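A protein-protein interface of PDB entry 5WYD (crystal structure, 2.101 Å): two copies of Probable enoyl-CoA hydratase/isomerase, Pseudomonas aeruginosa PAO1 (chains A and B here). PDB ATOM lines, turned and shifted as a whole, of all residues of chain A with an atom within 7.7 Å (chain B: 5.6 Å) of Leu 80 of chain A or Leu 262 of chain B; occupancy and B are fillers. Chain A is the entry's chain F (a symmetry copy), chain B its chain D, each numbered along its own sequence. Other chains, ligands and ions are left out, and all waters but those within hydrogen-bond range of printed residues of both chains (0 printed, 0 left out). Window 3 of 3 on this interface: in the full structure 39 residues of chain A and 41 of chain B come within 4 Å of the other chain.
Hydrophobic or aromatic side chains of chain A within 4 Å of the printed part of chain B: Leu 80 and Val 149. Of the 8 printed residues of chain B, 5 touch a printed residue of chain A. Hydrophobic or aromatic side chains of chain B that line the printed part of chain A: Val 258, Phe 261 and Leu 262. Among the printed residues, no Asp or Glu carboxylate lies within 4 Å of a Lys or Arg side-chain nitrogen of the other chain.
The side-chain amide oxygen (OD1) of Asn 259 of chain B sits close to the side-chain carboxylate (OD2) of Asp 85 of chain A, 2.6 Å away.
Of the printed residues of chain B, Leu 80 of chain A touches Phe 261 (3.3 Å) and Leu 262 (3.6 Å). Leu 262 of chain B touches just one residue of chain A: Leu 80 (3.6 Å). Printed residues of chain A within 4 Å of Phe 261 of chain B: Leu 80 (3.3 Å). Of the printed residues of chain B, Val 149 of chain A touches Gly 257 and Val 258. Of the printed residues of chain A, Asn 259 of chain B touches Asp 85 (2.6 Å). Glu 263 of chain B touches none of the printed residues of chain A. The nearest printed residue of chain B that does not touch Leu 80 of chain A is Val 258 of chain B (4.004 Å). The nearest residue of chain A that does not touch Leu 262 of chain B is Asn 81 of chain A (5.9 Å).
No position is printed for both chains. Of the 6 pairs that touch across the chains among the printed residues, none has its exchanged pair printed and touching as well.
Leu 80 of chain A touches Phe 261 of chain B. CD1 of Leu 262 of chain B touches CD1 of Leu 80 of chain A, at 3.6 Å. OD1 of Asp 85 of chain A touches CG1 of Val 258 of chain B, 3.3 Å away. CA of Gly 257 of chain B touches O of Val 149 of chain A (3.1 Å). Val 258 of chain B touches Val 149 of chain A.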
ATOM      1  N   THR A  39      26.011  16.446   7.689  1.00  0.00           N
ATOM      2  CA  THR A  39      25.635  16.096   9.041  1.00  0.00           C
ATOM      3  C   THR A  39      24.258  15.435   9.040  1.00  0.00           C
ATOM      4  O   THR A  39      23.388  15.771   8.228  1.00  0.00           O
ATOM      5  CB  THR A  39      25.694  17.341   9.917  1.00  0.00           C
ATOM      6  OG1 THR A  39      25.334  16.997  11.251  1.00  0.00           O
ATOM      7  CG2 THR A  39      24.738  18.407   9.379  1.00  0.00           C
ATOM      8  N   TRP A  40      24.097  14.442   9.925  1.00  0.00           N
ATOM      9  CA  TRP A  40      22.859  13.674  10.030  1.00  0.00           C
ATOM     10  C   TRP A  40      21.708  14.508  10.546  1.00  0.00           C
ATOM     11  O   TRP A  40      21.880  15.395  11.378  1.00  0.00           O
ATOM     12  CB  TRP A  40      23.026  12.491  10.970  1.00  0.00           C
ATOM     13  CG  TRP A  40      23.824  11.414  10.419  1.00  0.00           C
ATOM     14  CD1 TRP A  40      25.127  11.120  10.705  1.00  0.00           C
ATOM     15  CD2 TRP A  40      23.391  10.457   9.459  1.00  0.00           C
ATOM     16  NE1 TRP A  40      25.528  10.024   9.982  1.00  0.00           N
ATOM     17  CE2 TRP A  40      24.478   9.602   9.206  1.00  0.00           C
ATOM     18  CE3 TRP A  40      22.186  10.239   8.787  1.00  0.00           C
ATOM     19  CZ2 TRP A  40      24.394   8.550   8.315  1.00  0.00           C
ATOM     20  CZ3 TRP A  40      22.110   9.203   7.901  1.00  0.00           C
ATOM     21  CH2 TRP A  40      23.203   8.367   7.673  1.00  0.00           C
ATOM     22  N   GLY A  77      28.474  13.670  11.432  1.00  0.00           N
ATOM     23  CA  GLY A  77      27.784  13.332  12.642  1.00  0.00           C
ATOM     24  C   GLY A  77      26.423  14.010  12.680  1.00  0.00           C
ATOM     25  O   GLY A  77      25.851  14.434  11.669  1.00  0.00           O
ATOM     26  N   ALA A  78      25.888  14.079  13.886  1.00  0.00           N
ATOM     27  CA  ALA A  78      24.579  14.671  14.103  1.00  0.00           C
ATOM     28  C   ALA A  78      24.564  16.184  13.904  1.00  0.00           C
ATOM     29  O   ALA A  78      25.511  16.895  14.258  1.00  0.00           O
ATOM     30  CB  ALA A  78      24.109  14.320  15.504  1.00  0.00           C
ATOM     31  N   ASP A  79      23.488  16.670  13.301  1.00  0.00           N
ATOM     32  CA  ASP A  79      23.339  18.098  13.090  1.00  0.00           C
ATOM     33  C   ASP A  79      23.066  18.790  14.421  1.00  0.00           C
ATOM     34  O   ASP A  79      22.394  18.251  15.303  1.00  0.00           O
ATOM     35  CB  ASP A  79      22.218  18.353  12.088  1.00  0.00           C
ATOM     36  CG  ASP A  79      22.040  19.804  11.765  1.00  0.00           C
ATOM     37  OD1 ASP A  79      22.994  20.586  11.942  1.00  0.00           O
ATOM     38  OD2 ASP A  79      20.934  20.158  11.319  1.00  0.00           O
ATOM     39  N   LEU A  80      23.645  19.974  14.589  1.00  0.00           N
ATOM     40  CA  LEU A  80      23.452  20.713  15.832  1.00  0.00           C
ATOM     41  C   LEU A  80      22.016  21.178  16.006  1.00  0.00           C
ATOM     42  O   LEU A  80      21.503  21.194  17.134  1.00  0.00           O
ATOM     43  CB  LEU A  80      24.421  21.875  15.889  1.00  0.00           C
ATOM     44  CG  LEU A  80      25.808  21.301  16.103  1.00  0.00           C
ATOM     45  CD1 LEU A  80      26.771  22.456  16.064  1.00  0.00           C
ATOM     46  CD2 LEU A  80      25.834  20.552  17.450  1.00  0.00           C
ATOM     47  N   ASN A  81      21.351  21.571  14.911  1.00  0.00           N
ATOM     48  CA  ASN A  81      19.948  21.975  15.008  1.00  0.00           C
ATOM     49  C   ASN A  81      19.122  20.865  15.657  1.00  0.00           C
ATOM     50  O   ASN A  81      18.216  21.133  16.455  1.00  0.00           O
ATOM     51  CB  ASN A  81      19.355  22.298  13.630  1.00  0.00           C
ATOM     52  CG  ASN A  81      20.103  23.405  12.885  1.00  0.00           C
ATOM     53  OD1 ASN A  81      21.006  24.047  13.429  1.00  0.00           O
ATOM     54  ND2 ASN A  81      19.716  23.632  11.625  1.00  0.00           N
ATOM     55  N   MET A  82      19.451  19.610  15.338  1.00  0.00           N
ATOM     56  CA  MET A  82      18.746  18.472  15.906  1.00  0.00           C
ATOM     57  C   MET A  82      18.949  18.443  17.417  1.00  0.00           C
ATOM     58  O   MET A  82      18.003  18.198  18.176  1.00  0.00           O
ATOM     59  CB  MET A  82      19.246  17.221  15.165  1.00  0.00           C
ATOM     60  CG  MET A  82      18.592  15.891  15.384  1.00  0.00           C
ATOM     61  SD  MET A  82      19.146  14.913  13.979  1.00  0.00           S
ATOM     62  CE  MET A  82      18.426  13.346  14.425  1.00  0.00           C
ATOM     63  N   PHE A  83      20.151  18.773  17.882  1.00  0.00           N
ATOM     64  CA  PHE A  83      20.428  18.801  19.311  1.00  0.00           C
ATOM     65  C   PHE A  83      20.413  20.207  19.900  1.00  0.00           C
ATOM     66  O   PHE A  83      20.948  20.413  20.997  1.00  0.00           O
ATOM     67  CB  PHE A  83      21.744  18.095  19.622  1.00  0.00           C
ATOM     68  CG  PHE A  83      21.679  16.613  19.404  1.00  0.00           C
ATOM     69  CD1 PHE A  83      20.890  15.820  20.218  1.00  0.00           C
ATOM     70  CD2 PHE A  83      22.423  16.010  18.408  1.00  0.00           C
ATOM     71  CE1 PHE A  83      20.813  14.454  20.020  1.00  0.00           C
ATOM     72  CE2 PHE A  83      22.355  14.644  18.221  1.00  0.00           C
ATOM     73  CZ  PHE A  83      21.553  13.861  19.024  1.00  0.00           C
ATOM     74  N   ALA A  84      19.820  21.171  19.202  1.00  0.00           N
ATOM     75  CA  ALA A  84      19.808  22.530  19.707  1.00  0.00           C
ATOM     76  C   ALA A  84      19.189  22.544  21.085  1.00  0.00           C
ATOM     77  O   ALA A  84      18.187  21.871  21.341  1.00  0.00           O
ATOM     78  CB  ALA A  84      19.025  23.450  18.773  1.00  0.00           C
ATOM     79  N   ASP A  85      19.768  23.336  21.958  1.00  0.00           N
ATOM     80  CA  ASP A  85      19.273  23.341  23.298  1.00  0.00           C
ATOM     81  C   ASP A  85      17.859  23.868  23.307  1.00  0.00           C
ATOM     82  O   ASP A  85      17.459  24.612  22.420  1.00  0.00           O
ATOM     83  CB  ASP A  85      20.196  24.182  24.143  1.00  0.00           C
ATOM     84  CG  ASP A  85      21.609  23.787  23.948  1.00  0.00           C
ATOM     85  OD1 ASP A  85      21.862  23.159  22.901  1.00  0.00           O
ATOM     86  OD2 ASP A  85      22.434  24.028  24.850  1.00  0.00           O
ATOM     87  N   VAL A 149      31.660  17.626  24.266  1.00  0.00           N
ATOM     88  CA  VAL A 149      30.490  18.468  24.436  1.00  0.00           C
ATOM     89  C   VAL A 149      29.599  17.973  25.567  1.00  0.00           C
ATOM     90  O   VAL A 149      28.529  18.544  25.805  1.00  0.00           O
ATOM     91  CB  VAL A 149      29.731  18.542  23.104  1.00  0.00           C
ATOM     92  CG1 VAL A 149      30.730  18.649  21.954  1.00  0.00           C
ATOM     93  CG2 VAL A 149      28.900  17.320  22.944  1.00  0.00           C
ATOM     94  N   LEU A 151      28.095  14.975  25.733  1.00  0.00           N
ATOM     95  CA  LEU A 151      27.084  14.099  25.139  1.00  0.00           C
ATOM     96  C   LEU A 151      27.702  12.750  24.833  1.00  0.00           C
ATOM     97  O   LEU A 151      28.832  12.700  24.387  1.00  0.00           O
ATOM     98  CB  LEU A 151      26.553  14.692  23.840  1.00  0.00           C
ATOM     99  CG  LEU A 151      25.869  16.039  24.009  1.00  0.00           C
ATOM    100  CD1 LEU A 151      25.291  16.574  22.692  1.00  0.00           C
ATOM    101  CD2 LEU A 151      24.832  15.929  25.095  1.00  0.00           C
ATOM    102  N   GLY B 257      28.435  22.170  26.633  1.00  0.00           N
ATOM    103  CA  GLY B 257      29.291  21.575  25.616  1.00  0.00           C
ATOM    104  C   GLY B 257      28.821  21.828  24.191  1.00  0.00           C
ATOM    105  O   GLY B 257      29.621  22.149  23.306  1.00  0.00           O
ATOM    106  N   VAL B 258      27.519  21.661  23.946  1.00  0.00           N
ATOM    107  CA  VAL B 258      26.959  21.870  22.606  1.00  0.00           C
ATOM    108  C   VAL B 258      27.015  23.343  22.199  1.00  0.00           C
ATOM    109  O   VAL B 258      27.276  23.668  21.029  1.00  0.00           O
ATOM    110  CB  VAL B 258      25.531  21.295  22.526  1.00  0.00           C
ATOM    111  CG1 VAL B 258      24.694  21.745  23.725  1.00  0.00           C
ATOM    112  CG2 VAL B 258      24.888  21.642  21.185  1.00  0.00           C
ATOM    113  N   ASN B 259      26.722  24.253  23.139  1.00  0.00           N
ATOM    114  CA  ASN B 259      26.780  25.674  22.829  1.00  0.00           C
ATOM    115  C   ASN B 259      28.193  26.088  22.463  1.00  0.00           C
ATOM    116  O   ASN B 259      28.393  26.811  21.484  1.00  0.00           O
ATOM    117  CB  ASN B 259      26.296  26.492  24.026  1.00  0.00           C
ATOM    118  CG  ASN B 259      24.890  26.157  24.418  1.00  0.00           C
ATOM    119  OD1 ASN B 259      24.151  25.581  23.621  1.00  0.00           O
ATOM    120  ND2 ASN B 259      24.503  26.508  25.653  1.00  0.00           N
ATOM    121  N   ALA B 260      29.191  25.582  23.197  1.00  0.00           N
ATOM    122  CA  ALA B 260      30.574  25.966  22.943  1.00  0.00           C
ATOM    123  C   ALA B 260      31.003  25.593  21.532  1.00  0.00           C
ATOM    124  O   ALA B 260      31.658  26.383  20.847  1.00  0.00           O
ATOM    125  CB  ALA B 260      31.486  25.318  23.977  1.00  0.00           C
ATOM    126  N   PHE B 261      30.655  24.389  21.087  1.00  0.00           N
ATOM    127  CA  PHE B 261      30.964  24.002  19.721  1.00  0.00           C
ATOM    128  C   PHE B 261      30.246  24.880  18.721  1.00  0.00           C
ATOM    129  O   PHE B 261      30.771  25.183  17.646  1.00  0.00           O
ATOM    130  CB  PHE B 261      30.558  22.565  19.463  1.00  0.00           C
ATOM    131  CG  PHE B 261      30.833  22.126  18.053  1.00  0.00           C
ATOM    132  CD1 PHE B 261      32.076  21.651  17.691  1.00  0.00           C
ATOM    133  CD2 PHE B 261      29.853  22.221  17.078  1.00  0.00           C
ATOM    134  CE1 PHE B 261      32.318  21.259  16.390  1.00  0.00           C
ATOM    135  CE2 PHE B 261      30.089  21.836  15.773  1.00  0.00           C
ATOM    136  CZ  PHE B 261      31.318  21.357  15.427  1.00  0.00           C
ATOM    137  N   LEU B 262      29.010  25.219  19.012  1.00  0.00           N
ATOM    138  CA  LEU B 262      28.278  26.021  18.067  1.00  0.00           C
ATOM    139  C   LEU B 262      28.958  27.381  17.888  1.00  0.00           C
ATOM    140  O   LEU B 262      29.113  27.850  16.759  1.00  0.00           O
ATOM    141  CB  LEU B 262      26.834  26.107  18.552  1.00  0.00           C
ATOM    142  CG  LEU B 262      25.791  26.719  17.646  1.00  0.00           C
ATOM    143  CD1 LEU B 262      25.731  25.853  16.398  1.00  0.00           C
ATOM    144  CD2 LEU B 262      24.442  26.779  18.402  1.00  0.00           C
ATOM    145  N   GLU B 263      29.414  28.005  18.987  1.00  0.00           N
ATOM    146  CA  GLU B 263      30.087  29.307  18.973  1.00  0.00           C
ATOM    147  C   GLU B 263      31.609  29.237  18.839  1.00  0.00           C
ATOM    148  O   GLU B 263      32.284  30.239  19.099  1.00  0.00           O
ATOM    149  CB  GLU B 263      29.726  30.063  20.244  1.00  0.00           C
ATOM    150  CG  GLU B 263      29.875  29.193  21.440  1.00  0.00           C
ATOM    151  CD  GLU B 263      29.063  29.633  22.631  1.00  0.00           C
ATOM    152  OE1 GLU B 263      28.326  30.637  22.556  1.00  0.00           O
ATOM    153  OE2 GLU B 263      29.118  28.918  23.650  1.00  0.00           O
ATOM    154  N   LYS B 264      32.173  28.087  18.495  1.00  0.00           N
ATOM    155  CA  LYS B 264      33.610  27.956  18.243  1.00  0.00           C
ATOM    156  C   LYS B 264      34.443  28.318  19.487  1.00  0.00           C
ATOM    157  O   LYS B 264      35.612  28.716  19.408  1.00  0.00           O
ATOM    158  CB  LYS B 264      34.025  28.768  17.005  1.00  0.00           C
ATOM    159  CG  LYS B 264      33.349  28.492  15.701  1.00  0.00           C
ATOM    160  CD  LYS B 264      33.591  27.340  15.132  1.00  0.00           C
ATOM    161  CE  LYS B 264      32.452  26.296  15.227  1.00  0.00           C
ATOM    162  NZ  LYS B 264      33.165  24.955  14.648  1.00  0.00           N
